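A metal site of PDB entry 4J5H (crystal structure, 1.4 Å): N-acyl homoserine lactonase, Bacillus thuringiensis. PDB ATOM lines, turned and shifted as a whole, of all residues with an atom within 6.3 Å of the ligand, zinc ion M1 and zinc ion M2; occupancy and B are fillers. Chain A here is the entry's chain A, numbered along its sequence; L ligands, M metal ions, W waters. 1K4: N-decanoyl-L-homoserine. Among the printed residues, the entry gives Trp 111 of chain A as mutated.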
ATOM      1  N   CYS A  18     -18.102 -21.407 -14.152  1.00  0.00           N
ATOM      2  CA  CYS A  18     -18.665 -22.343 -13.208  1.00  0.00           C
ATOM      3  C   CYS A  18     -17.837 -23.610 -13.179  1.00  0.00           C
ATOM      4  O   CYS A  18     -17.353 -24.075 -14.207  1.00  0.00           O
ATOM      5  CB  CYS A  18     -20.136 -22.645 -13.490  1.00  0.00           C
ATOM      6  SG  CYS A  18     -20.475 -23.430 -15.076  1.00  0.00           S
ATOM      7  N   MET A  19     -17.688 -24.145 -11.964  1.00  0.00           N
ATOM      8  CA  MET A  19     -17.024 -25.414 -11.777  1.00  0.00           C
ATOM      9  C   MET A  19     -18.057 -26.477 -11.999  1.00  0.00           C
ATOM     10  O   MET A  19     -19.174 -26.391 -11.487  1.00  0.00           O
ATOM     11  CB  MET A  19     -16.504 -25.605 -10.357  1.00  0.00           C
ATOM     12  CG  MET A  19     -15.637 -24.494  -9.842  1.00  0.00           C
ATOM     13  SD  MET A  19     -14.125 -24.167 -10.800  1.00  0.00           S
ATOM     14  CE  MET A  19     -13.360 -25.775 -10.749  1.00  0.00           C
ATOM     15  N   LEU A  20     -17.671 -27.487 -12.761  1.00  0.00           N
ATOM     16  CA  LEU A  20     -18.520 -28.610 -13.089  1.00  0.00           C
ATOM     17  C   LEU A  20     -17.691 -29.887 -13.032  1.00  0.00           C
ATOM     18  O   LEU A  20     -16.589 -29.962 -13.582  1.00  0.00           O
ATOM     19  CB  LEU A  20     -19.110 -28.463 -14.495  1.00  0.00           C
ATOM     20  CG  LEU A  20     -20.050 -29.555 -14.984  1.00  0.00           C
ATOM     21  CD1 LEU A  20     -21.247 -29.721 -14.068  1.00  0.00           C
ATOM     22  CD2 LEU A  20     -20.500 -29.210 -16.408  1.00  0.00           C
ATOM     23  N   LEU A  37     -15.221 -23.971 -16.085  1.00  0.00           N
ATOM     24  CA  LEU A  37     -15.727 -23.806 -17.447  1.00  0.00           C
ATOM     25  C   LEU A  37     -16.228 -22.407 -17.666  1.00  0.00           C
ATOM     26  O   LEU A  37     -16.721 -21.785 -16.721  1.00  0.00           O
ATOM     27  CB  LEU A  37     -16.905 -24.731 -17.681  1.00  0.00           C
ATOM     28  CG  LEU A  37     -16.646 -26.218 -17.576  1.00  0.00           C
ATOM     29  CD1 LEU A  37     -17.956 -26.939 -17.836  1.00  0.00           C
ATOM     30  CD2 LEU A  37     -15.569 -26.614 -18.546  1.00  0.00           C
ATOM     31  N   PHE A  68     -25.392 -24.249  -4.536  1.00  0.00           N
ATOM     32  CA  PHE A  68     -26.098 -25.519  -4.697  1.00  0.00           C
ATOM     33  C   PHE A  68     -25.890 -26.484  -3.551  1.00  0.00           C
ATOM     34  O   PHE A  68     -26.247 -27.664  -3.631  1.00  0.00           O
ATOM     35  CB  PHE A  68     -25.751 -26.147  -6.037  1.00  0.00           C
ATOM     36  CG  PHE A  68     -26.218 -25.319  -7.188  1.00  0.00           C
ATOM     37  CD1 PHE A  68     -27.555 -24.954  -7.326  1.00  0.00           C
ATOM     38  CD2 PHE A  68     -25.302 -24.827  -8.099  1.00  0.00           C
ATOM     39  CE1 PHE A  68     -27.961 -24.133  -8.392  1.00  0.00           C
ATOM     40  CE2 PHE A  68     -25.725 -24.025  -9.164  1.00  0.00           C
ATOM     41  CZ  PHE A  68     -27.037 -23.672  -9.299  1.00  0.00           C
ATOM     42  N   THR A  71     -28.677 -29.335  -2.339  1.00  0.00           N
ATOM     43  CA  THR A  71     -29.442 -29.735  -3.521  1.00  0.00           C
ATOM     44  C   THR A  71     -28.836 -30.991  -4.112  1.00  0.00           C
ATOM     45  O   THR A  71     -27.748 -31.427  -3.694  1.00  0.00           O
ATOM     46  CB  THR A  71     -29.395 -28.668  -4.633  1.00  0.00           C
ATOM     47  OG1 THR A  71     -28.120 -28.700  -5.285  1.00  0.00           O
ATOM     48  CG2 THR A  71     -29.656 -27.269  -4.069  1.00  0.00           C
ATOM     49  N   PHE A  72     -29.509 -31.541  -5.116  1.00  0.00           N
ATOM     50  CA  PHE A  72     -29.072 -32.778  -5.754  1.00  0.00           C
ATOM     51  C   PHE A  72     -27.751 -32.643  -6.539  1.00  0.00           C
ATOM     52  O   PHE A  72     -27.176 -33.646  -6.938  1.00  0.00           O
ATOM     53  CB  PHE A  72     -30.197 -33.386  -6.630  1.00  0.00           C
ATOM     54  CG  PHE A  72     -30.506 -32.592  -7.884  1.00  0.00           C
ATOM     55  CD1 PHE A  72     -31.315 -31.461  -7.820  1.00  0.00           C
ATOM     56  CD2 PHE A  72     -30.014 -33.011  -9.122  1.00  0.00           C
ATOM     57  CE1 PHE A  72     -31.587 -30.736  -8.975  1.00  0.00           C
ATOM     58  CE2 PHE A  72     -30.299 -32.280 -10.278  1.00  0.00           C
ATOM     59  CZ  PHE A  72     -31.083 -31.144 -10.199  1.00  0.00           C
ATOM     60  N   VAL A  73     -27.257 -31.409  -6.732  1.00  0.00           N
ATOM     61  CA  VAL A  73     -25.963 -31.183  -7.399  1.00  0.00           C
ATOM     62  C   VAL A  73     -24.873 -30.590  -6.475  1.00  0.00           C
ATOM     63  O   VAL A  73     -23.832 -30.116  -6.974  1.00  0.00           O
ATOM     64  CB  VAL A  73     -26.138 -30.313  -8.651  1.00  0.00           C
ATOM     65  CG1 VAL A  73     -27.184 -30.915  -9.579  1.00  0.00           C
ATOM     66  CG2 VAL A  73     -26.523 -28.890  -8.284  1.00  0.00           C
ATOM     67  N   ILE A  77     -21.523 -28.640  -8.990  1.00  0.00           N
ATOM     68  CA  ILE A  77     -21.657 -27.366  -9.707  1.00  0.00           C
ATOM     69  C   ILE A  77     -21.390 -26.251  -8.711  1.00  0.00           C
ATOM     70  O   ILE A  77     -22.103 -26.150  -7.697  1.00  0.00           O
ATOM     71  CB  ILE A  77     -23.076 -27.173 -10.301  1.00  0.00           C
ATOM     72  CG1 ILE A  77     -23.423 -28.316 -11.266  1.00  0.00           C
ATOM     73  CG2 ILE A  77     -23.162 -25.829 -10.984  1.00  0.00           C
ATOM     74  CD1 ILE A  77     -24.769 -28.200 -11.959  1.00  0.00           C
ATOM     75  N   HIS A 108     -31.871 -21.905 -23.719  1.00  0.00           N
ATOM     76  CA  HIS A 108     -32.602 -22.694 -22.822  1.00  0.00           C
ATOM     77  C   HIS A 108     -32.608 -21.984 -21.464  1.00  0.00           C
ATOM     78  O   HIS A 108     -31.983 -20.925 -21.312  1.00  0.00           O
ATOM     79  CB  HIS A 108     -32.073 -24.126 -22.774  1.00  0.00           C
ATOM     80  CG  HIS A 108     -30.688 -24.319 -22.255  1.00  0.00           C
ATOM     81  ND1 HIS A 108     -29.574 -23.628 -22.700  1.00  0.00           N
ATOM     82  CD2 HIS A 108     -30.226 -25.253 -21.403  1.00  0.00           C
ATOM     83  CE1 HIS A 108     -28.495 -24.136 -22.126  1.00  0.00           C
ATOM     84  NE2 HIS A 108     -28.869 -25.116 -21.332  1.00  0.00           N
ATOM     85  N   HIS A 110     -31.701 -23.233 -18.340  1.00  0.00           N
ATOM     86  CA  HIS A 110     -30.747 -23.602 -17.311  1.00  0.00           C
ATOM     87  C   HIS A 110     -30.136 -22.375 -16.636  1.00  0.00           C
ATOM     88  O   HIS A 110     -30.074 -21.303 -17.224  1.00  0.00           O
ATOM     89  CB  HIS A 110     -29.671 -24.545 -17.849  1.00  0.00           C
ATOM     90  CG  HIS A 110     -30.171 -25.930 -18.126  1.00  0.00           C
ATOM     91  ND1 HIS A 110     -29.468 -26.832 -18.891  1.00  0.00           N
ATOM     92  CD2 HIS A 110     -31.288 -26.570 -17.719  1.00  0.00           C
ATOM     93  CE1 HIS A 110     -30.149 -27.972 -18.943  1.00  0.00           C
ATOM     94  NE2 HIS A 110     -31.269 -27.832 -18.264  1.00  0.00           N
ATOM     95  N   TRP A 111     -29.684 -22.589 -15.410  1.00  0.00           N
ATOM     96  CA  TRP A 111     -29.393 -21.528 -14.447  1.00  0.00           C
ATOM     97  C   TRP A 111     -28.334 -20.536 -14.906  1.00  0.00           C
ATOM     98  O   TRP A 111     -28.365 -19.372 -14.536  1.00  0.00           O
ATOM     99  CB  TRP A 111     -29.055 -22.149 -13.072  1.00  0.00           C
ATOM    100  CG  TRP A 111     -27.690 -22.765 -13.070  1.00  0.00           C
ATOM    101  CD1 TRP A 111     -27.321 -23.976 -13.594  1.00  0.00           C
ATOM    102  CD2 TRP A 111     -26.496 -22.136 -12.634  1.00  0.00           C
ATOM    103  NE1 TRP A 111     -25.964 -24.148 -13.484  1.00  0.00           N
ATOM    104  CE2 TRP A 111     -25.428 -23.036 -12.894  1.00  0.00           C
ATOM    105  CE3 TRP A 111     -26.214 -20.909 -12.012  1.00  0.00           C
ATOM    106  CZ2 TRP A 111     -24.105 -22.736 -12.571  1.00  0.00           C
ATOM    107  CZ3 TRP A 111     -24.895 -20.634 -11.686  1.00  0.00           C
ATOM    108  CH2 TRP A 111     -23.859 -21.539 -11.983  1.00  0.00           C
ATOM    109  N   ASP A 112     -27.375 -21.026 -15.677  1.00  0.00           N
ATOM    110  CA  ASP A 112     -26.253 -20.244 -16.161  1.00  0.00           C
ATOM    111  C   ASP A 112     -26.480 -19.657 -17.550  1.00  0.00           C
ATOM    112  O   ASP A 112     -25.574 -19.018 -18.112  1.00  0.00           O
ATOM    113  CB  ASP A 112     -24.927 -21.005 -16.085  1.00  0.00           C
ATOM    114  CG  ASP A 112     -24.931 -22.291 -16.889  1.00  0.00           C
ATOM    115  OD1 ASP A 112     -25.957 -22.990 -16.986  1.00  0.00           O
ATOM    116  OD2 ASP A 112     -23.859 -22.640 -17.401  1.00  0.00           O
ATOM    117  N   HIS A 113     -27.682 -19.872 -18.069  1.00  0.00           N
ATOM    118  CA  HIS A 113     -28.115 -19.330 -19.360  1.00  0.00           C
ATOM    119  C   HIS A 113     -29.281 -18.336 -19.270  1.00  0.00           C
ATOM    120  O   HIS A 113     -29.389 -17.442 -20.121  1.00  0.00           O
ATOM    121  CB  HIS A 113     -28.487 -20.442 -20.315  1.00  0.00           C
ATOM    122  CG  HIS A 113     -27.334 -21.283 -20.669  1.00  0.00           C
ATOM    123  ND1 HIS A 113     -26.549 -21.034 -21.770  1.00  0.00           N
ATOM    124  CD2 HIS A 113     -26.804 -22.353 -20.045  1.00  0.00           C
ATOM    125  CE1 HIS A 113     -25.558 -21.905 -21.778  1.00  0.00           C
ATOM    126  NE2 HIS A 113     -25.715 -22.733 -20.762  1.00  0.00           N
ATOM    127  N   GLU A 139     -37.076 -30.140 -11.704  1.00  0.00           N
ATOM    128  CA  GLU A 139     -36.276 -29.736 -10.543  1.00  0.00           C
ATOM    129  C   GLU A 139     -34.973 -29.015 -10.879  1.00  0.00           C
ATOM    130  O   GLU A 139     -34.430 -28.323 -10.042  1.00  0.00           O
ATOM    131  CB  GLU A 139     -35.963 -30.925  -9.641  1.00  0.00           C
ATOM    132  CG  GLU A 139     -35.093 -31.995 -10.279  1.00  0.00           C
ATOM    133  CD  GLU A 139     -34.990 -33.263  -9.421  1.00  0.00           C
ATOM    134  OE1 GLU A 139     -34.396 -34.254  -9.887  1.00  0.00           O
ATOM    135  OE2 GLU A 139     -35.512 -33.251  -8.280  1.00  0.00           O
ATOM    136  N   GLU A 140     -34.460 -29.215 -12.090  1.00  0.00           N
ATOM    137  CA  GLU A 140     -33.198 -28.583 -12.485  1.00  0.00           C
ATOM    138  C   GLU A 140     -33.342 -27.102 -12.874  1.00  0.00           C
ATOM    139  O   GLU A 140     -32.376 -26.485 -13.332  1.00  0.00           O
ATOM    140  CB  GLU A 140     -32.488 -29.384 -13.594  1.00  0.00           C
ATOM    141  CG  GLU A 140     -33.148 -29.401 -14.968  1.00  0.00           C
ATOM    142  CD  GLU A 140     -34.168 -30.498 -15.174  1.00  0.00           C
ATOM    143  OE1 GLU A 140     -34.487 -30.783 -16.353  1.00  0.00           O
ATOM    144  OE2 GLU A 140     -34.652 -31.110 -14.177  1.00  0.00           O
ATOM    145  N   TYR A 141     -34.550 -26.547 -12.736  1.00  0.00           N
ATOM    146  CA  TYR A 141     -34.789 -25.132 -13.036  1.00  0.00           C
ATOM    147  C   TYR A 141     -34.952 -24.279 -11.794  1.00  0.00           C
ATOM    148  O   TYR A 141     -35.744 -24.619 -10.885  1.00  0.00           O
ATOM    149  CB  TYR A 141     -35.999 -24.968 -13.942  1.00  0.00           C
ATOM    150  CG  TYR A 141     -35.729 -25.566 -15.330  1.00  0.00           C
ATOM    151  CD1 TYR A 141     -35.111 -24.809 -16.303  1.00  0.00           C
ATOM    152  CD2 TYR A 141     -36.028 -26.900 -15.614  1.00  0.00           C
ATOM    153  CE1 TYR A 141     -34.846 -25.345 -17.527  1.00  0.00           C
ATOM    154  CE2 TYR A 141     -35.776 -27.448 -16.853  1.00  0.00           C
ATOM    155  CZ  TYR A 141     -35.208 -26.648 -17.817  1.00  0.00           C
ATOM    156  OH  TYR A 141     -34.898 -27.159 -19.052  1.00  0.00           O
ATOM    157  N   MET A 142     -34.174 -23.199 -11.752  1.00  0.00           N
ATOM    158  CA  MET A 142     -34.234 -22.246 -10.653  1.00  0.00           C
ATOM    159  C   MET A 142     -35.366 -21.269 -10.905  1.00  0.00           C
ATOM    160  O   MET A 142     -35.633 -20.928 -12.062  1.00  0.00           O
ATOM    161  CB  MET A 142     -32.913 -21.466 -10.552  1.00  0.00           C
ATOM    162  CG  MET A 142     -31.689 -22.287 -10.194  1.00  0.00           C
ATOM    163  SD  MET A 142     -30.256 -21.265  -9.865  1.00  0.00           S
ATOM    164  CE  MET A 142     -30.611 -20.490  -8.303  1.00  0.00           C
ATOM    165  N   HIS A 173     -30.495 -32.016 -24.577  1.00  0.00           N
ATOM    166  CA  HIS A 173     -29.775 -31.552 -23.421  1.00  0.00           C
ATOM    167  C   HIS A 173     -30.758 -30.976 -22.393  1.00  0.00           C
ATOM    168  O   HIS A 173     -30.608 -31.176 -21.162  1.00  0.00           O
ATOM    169  CB  HIS A 173     -28.695 -30.541 -23.802  1.00  0.00           C
ATOM    170  CG  HIS A 173     -28.174 -29.778 -22.642  1.00  0.00           C
ATOM    171  ND1 HIS A 173     -27.313 -30.311 -21.690  1.00  0.00           N
ATOM    172  CD2 HIS A 173     -28.465 -28.526 -22.247  1.00  0.00           C
ATOM    173  CE1 HIS A 173     -27.104 -29.401 -20.758  1.00  0.00           C
ATOM    174  NE2 HIS A 173     -27.773 -28.307 -21.092  1.00  0.00           N
ATOM    175  N   SER A 174     -31.726 -30.192 -22.918  1.00  0.00           N
ATOM    176  CA  SER A 174     -32.900 -29.774 -22.171  1.00  0.00           C
ATOM    177  C   SER A 174     -34.103 -29.957 -23.075  1.00  0.00           C
ATOM    178  O   SER A 174     -33.943 -30.146 -24.270  1.00  0.00           O
ATOM    179  CB  SER A 174     -32.768 -28.336 -21.726  1.00  0.00           C
ATOM    180  OG  SER A 174     -32.861 -27.416 -22.813  1.00  0.00           O
ATOM    181  N   HIS A 177     -34.156 -27.066 -25.839  1.00  0.00           N
ATOM    182  CA  HIS A 177     -32.922 -26.403 -26.166  1.00  0.00           C
ATOM    183  C   HIS A 177     -32.936 -25.970 -27.640  1.00  0.00           C
ATOM    184  O   HIS A 177     -33.404 -26.708 -28.512  1.00  0.00           O
ATOM    185  CB  HIS A 177     -31.732 -27.338 -25.901  1.00  0.00           C
ATOM    186  CG  HIS A 177     -30.414 -26.691 -26.109  1.00  0.00           C
ATOM    187  ND1 HIS A 177     -29.828 -26.561 -27.349  1.00  0.00           N
ATOM    188  CD2 HIS A 177     -29.618 -26.030 -25.246  1.00  0.00           C
ATOM    189  CE1 HIS A 177     -28.718 -25.867 -27.231  1.00  0.00           C
ATOM    190  NE2 HIS A 177     -28.574 -25.534 -25.953  1.00  0.00           N
ATOM    191  N   ILE A 194     -24.447 -23.913 -28.542  1.00  0.00           N
ATOM    192  CA  ILE A 194     -24.765 -23.782 -27.113  1.00  0.00           C
ATOM    193  C   ILE A 194     -24.633 -25.151 -26.472  1.00  0.00           C
ATOM    194  O   ILE A 194     -23.654 -25.836 -26.750  1.00  0.00           O
ATOM    195  CB  ILE A 194     -26.093 -23.034 -26.837  1.00  0.00           C
ATOM    196  CG1 ILE A 194     -26.340 -21.922 -27.860  1.00  0.00           C
ATOM    197  CG2 ILE A 194     -26.088 -22.494 -25.401  1.00  0.00           C
ATOM    198  CD1 ILE A 194     -25.442 -20.731 -27.727  1.00  0.00           C
ATOM    199  N   ASP A 195     -25.570 -25.571 -25.641  1.00  0.00           N
ATOM    200  CA  ASP A 195     -25.428 -26.812 -24.909  1.00  0.00           C
ATOM    201  C   ASP A 195     -25.948 -28.047 -25.677  1.00  0.00           C
ATOM    202  O   ASP A 195     -26.066 -29.118 -25.091  1.00  0.00           O
ATOM    203  CB  ASP A 195     -26.102 -26.719 -23.542  1.00  0.00           C
ATOM    204  CG  ASP A 195     -25.372 -25.806 -22.560  1.00  0.00           C
ATOM    205  OD1 ASP A 195     -24.384 -25.182 -22.945  1.00  0.00           O
ATOM    206  OD2 ASP A 195     -25.823 -25.696 -21.394  1.00  0.00           O
ATOM    207  N   TYR A 198     -21.408 -29.449 -25.178  1.00  0.00           N
ATOM    208  CA  TYR A 198     -20.544 -28.666 -24.312  1.00  0.00           C
ATOM    209  C   TYR A 198     -19.175 -28.475 -24.940  1.00  0.00           C
ATOM    210  O   TYR A 198     -18.606 -27.398 -24.880  1.00  0.00           O
ATOM    211  CB  TYR A 198     -20.361 -29.332 -22.953  1.00  0.00           C
ATOM    212  CG  TYR A 198     -21.486 -29.296 -21.964  1.00  0.00           C
ATOM    213  CD1 TYR A 198     -22.613 -28.505 -22.140  1.00  0.00           C
ATOM    214  CD2 TYR A 198     -21.391 -30.025 -20.796  1.00  0.00           C
ATOM    215  CE1 TYR A 198     -23.596 -28.459 -21.172  1.00  0.00           C
ATOM    216  CE2 TYR A 198     -22.357 -29.990 -19.814  1.00  0.00           C
ATOM    217  CZ  TYR A 198     -23.464 -29.208 -20.000  1.00  0.00           C
ATOM    218  OH  TYR A 198     -24.442 -29.166 -19.019  1.00  0.00           O
ATOM    219  N   ALA A 210     -23.897 -34.411 -19.952  1.00  0.00           N
ATOM    220  CA  ALA A 210     -25.103 -34.254 -19.162  1.00  0.00           C
ATOM    221  C   ALA A 210     -26.265 -33.765 -20.010  1.00  0.00           C
ATOM    222  O   ALA A 210     -26.125 -32.792 -20.801  1.00  0.00           O
ATOM    223  CB  ALA A 210     -24.863 -33.297 -18.030  1.00  0.00           C
ATOM    224  N   GLY A 238     -20.552 -25.033 -26.345  1.00  0.00           N
ATOM    225  CA  GLY A 238     -21.157 -24.334 -25.189  1.00  0.00           C
ATOM    226  C   GLY A 238     -20.277 -24.004 -24.003  1.00  0.00           C
ATOM    227  O   GLY A 238     -20.370 -22.912 -23.410  1.00  0.00           O
ATOM    228  N   HIS A 239     -19.419 -24.954 -23.644  1.00  0.00           N
ATOM    229  CA  HIS A 239     -18.533 -24.816 -22.448  1.00  0.00           C
ATOM    230  C   HIS A 239     -17.240 -25.568 -22.704  1.00  0.00           C
ATOM    231  O   HIS A 239     -16.996 -26.644 -22.103  1.00  0.00           O
ATOM    232  CB  HIS A 239     -19.195 -25.363 -21.188  1.00  0.00           C
ATOM    233  CG  HIS A 239     -20.519 -24.740 -20.856  1.00  0.00           C
ATOM    234  ND1 HIS A 239     -20.631 -23.485 -20.301  1.00  0.00           N
ATOM    235  CD2 HIS A 239     -21.795 -25.196 -20.978  1.00  0.00           C
ATOM    236  CE1 HIS A 239     -21.901 -23.199 -20.086  1.00  0.00           C
ATOM    237  NE2 HIS A 239     -22.632 -24.214 -20.506  1.00  0.00           N
HETATM  238  O   1K4 L   1     -26.588 -26.407 -18.689  1.00  0.00           O
HETATM  239  C   1K4 L   1     -25.651 -25.813 -18.140  1.00  0.00           C
HETATM  240  OXT 1K4 L   1     -25.004 -24.914 -18.780  1.00  0.00           O
HETATM  241  CA  1K4 L   1     -25.310 -26.201 -16.718  1.00  0.00           C
HETATM  242  CB  1K4 L   1     -23.789 -26.475 -16.711  1.00  0.00           C
HETATM  243  CAG 1K4 L   1     -23.161 -26.507 -15.339  1.00  0.00           C
HETATM  244  OAD 1K4 L   1     -23.489 -25.297 -14.650  1.00  0.00           O
HETATM  245  N   1K4 L   1     -25.964 -27.448 -16.292  1.00  0.00           N
HETATM  246  CAQ 1K4 L   1     -27.222 -27.401 -15.847  1.00  0.00           C
HETATM  247  OAB 1K4 L   1     -27.875 -26.357 -15.697  1.00  0.00           O
HETATM  248  CAN 1K4 L   1     -27.852 -28.709 -15.496  1.00  0.00           C
HETATM  249  CAM 1K4 L   1     -28.846 -28.607 -14.349  1.00  0.00           C
HETATM  250  CAL 1K4 L   1     -28.121 -28.223 -13.070  1.00  0.00           C
HETATM  251  CAK 1K4 L   1     -29.029 -28.288 -11.849  1.00  0.00           C
HETATM  252  CAJ 1K4 L   1     -29.275 -26.929 -11.232  1.00  0.00           C
HETATM  253  CAI 1K4 L   1     -29.972 -27.120  -9.880  1.00  0.00           C
HETATM  254  CAH 1K4 L   1     -31.172 -26.187  -9.739  1.00  0.00           C
HETATM  255  CAF 1K4 L   1     -31.591 -25.919  -8.284  1.00  0.00           C
HETATM  256  CAA 1K4 L   1     -31.634 -27.160  -7.424  1.00  0.00           C
HETATM  257 ZN    ZN M   1     -27.768 -26.465 -20.172  1.00  0.00          ZN
HETATM  258 ZN    ZN M   2     -24.645 -24.422 -20.460  1.00  0.00          ZN
HETATM  259  O   HOH W   1     -30.342 -25.327 -14.595  1.00  0.00           O
HETATM  260  O   HOH W   2     -24.307 -30.310 -16.311  1.00  0.00           O
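OAD of the ligand sits at hydrogen-bond distance from SG of Cys 18, 3.6 Å away. NE1 of Trp 111 lies within hydrogen-bond range of OAD of the ligand, at 3.0 Å.
N of Asp 195 is in hydrogen-bond range of NE2 of His 177 (3.0 Å). N of Leu 37 is in hydrogen-bond range of O of Cys 18. OG1 of Thr 71 lies close to N of Val 73 (3.2 Å). O of Tyr 198 sits at hydrogen-bond distance from N of Gly 238. O of Tyr 198 is in hydrogen-bond range of N of His 239 (2.9 Å). OG1 of Thr 71 is in hydrogen-bond range of O of Phe 68 (2.7 Å). The backbone carbonyl oxygen of Ala 210 lies within hydrogen-bond range of a ring nitrogen (ND1) of His 173.
OD1 of Asp 112 lies close to OXT of the ligand, 2.8 Å away. Leu 20 touches the ligand. Phe 68 touches the ligand. Thr 71 touches the ligand. Phe 72 touches the ligand (CZ to CAK, 3.9 Å). Val 73 touches the ligand. CD1 of Ile 77 touches CAL of the ligand, 3.5 Å away. O of Glu 139 touches CAH of the ligand, at 3.9 Å. Glu 140 touches the ligand. Met 142 touches the ligand (CG to CAH, 3.96 Å). Tyr 198 touches the ligand. Within 4 Å of the ligand: Cys 18, Leu 20, Phe 68, Thr 71, Phe 72, Val 73, Ile 77, His 108, His 110, Trp 111, Asp 112, His 113, Glu 139, Glu 140, Met 142, His 173, Asp 195, Tyr 198 and His 239.
Of the 27 residues printed, 4 come within 4 Å of zinc ion M1. The nearest printed residue that does not touch zinc ion M1 is His 113 (4.2 Å).
OD2 of Asp 112 touches zinc ion M2 (3.6 Å). Four residues have an atom within 4 Å of zinc ion M2: Asp 112, His 113, Asp 195 and His 239. The nearest printed residue that does not touch zinc ion M2 is His 108 (4.2 Å).
Zinc ion M1 is bound by an oxygen (O) of the ligand (1.9 Å), a ring nitrogen (NE2) of His 173 (2.1 Å), a ring nitrogen (NE2) of His 108 (2.1 Å), a ring nitrogen (ND1) of His 110 (2.2 Å) and the side-chain carboxylate of Asp 195 (2.4 Å).
OXT of the ligand is bound to zinc ion M2, at 1.8 Å. OD2 of Asp 195 is bound to zinc ion M2 (2.0 Å). Zinc ion M2 is bound by NE2 of His 113 (2.0 Å). Zinc ion M2 is bound by NE2 of His 239 (2.0 Å). Slightly farther from zinc ion M2 lies OD1 of Asp 195 (2.6 Å).
Water W1 lies within hydrogen-bond range of the backbone carbonyl oxygen of Glu 140 (2.7 Å), an oxygen (OAB) of the ligand (2.9 Å) and the backbone NH of Trp 111 (2.9 Å). Water W2 lies within hydrogen-bond range of OH of Tyr 198 (2.9 Å) and N of the ligand (3.3 Å).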
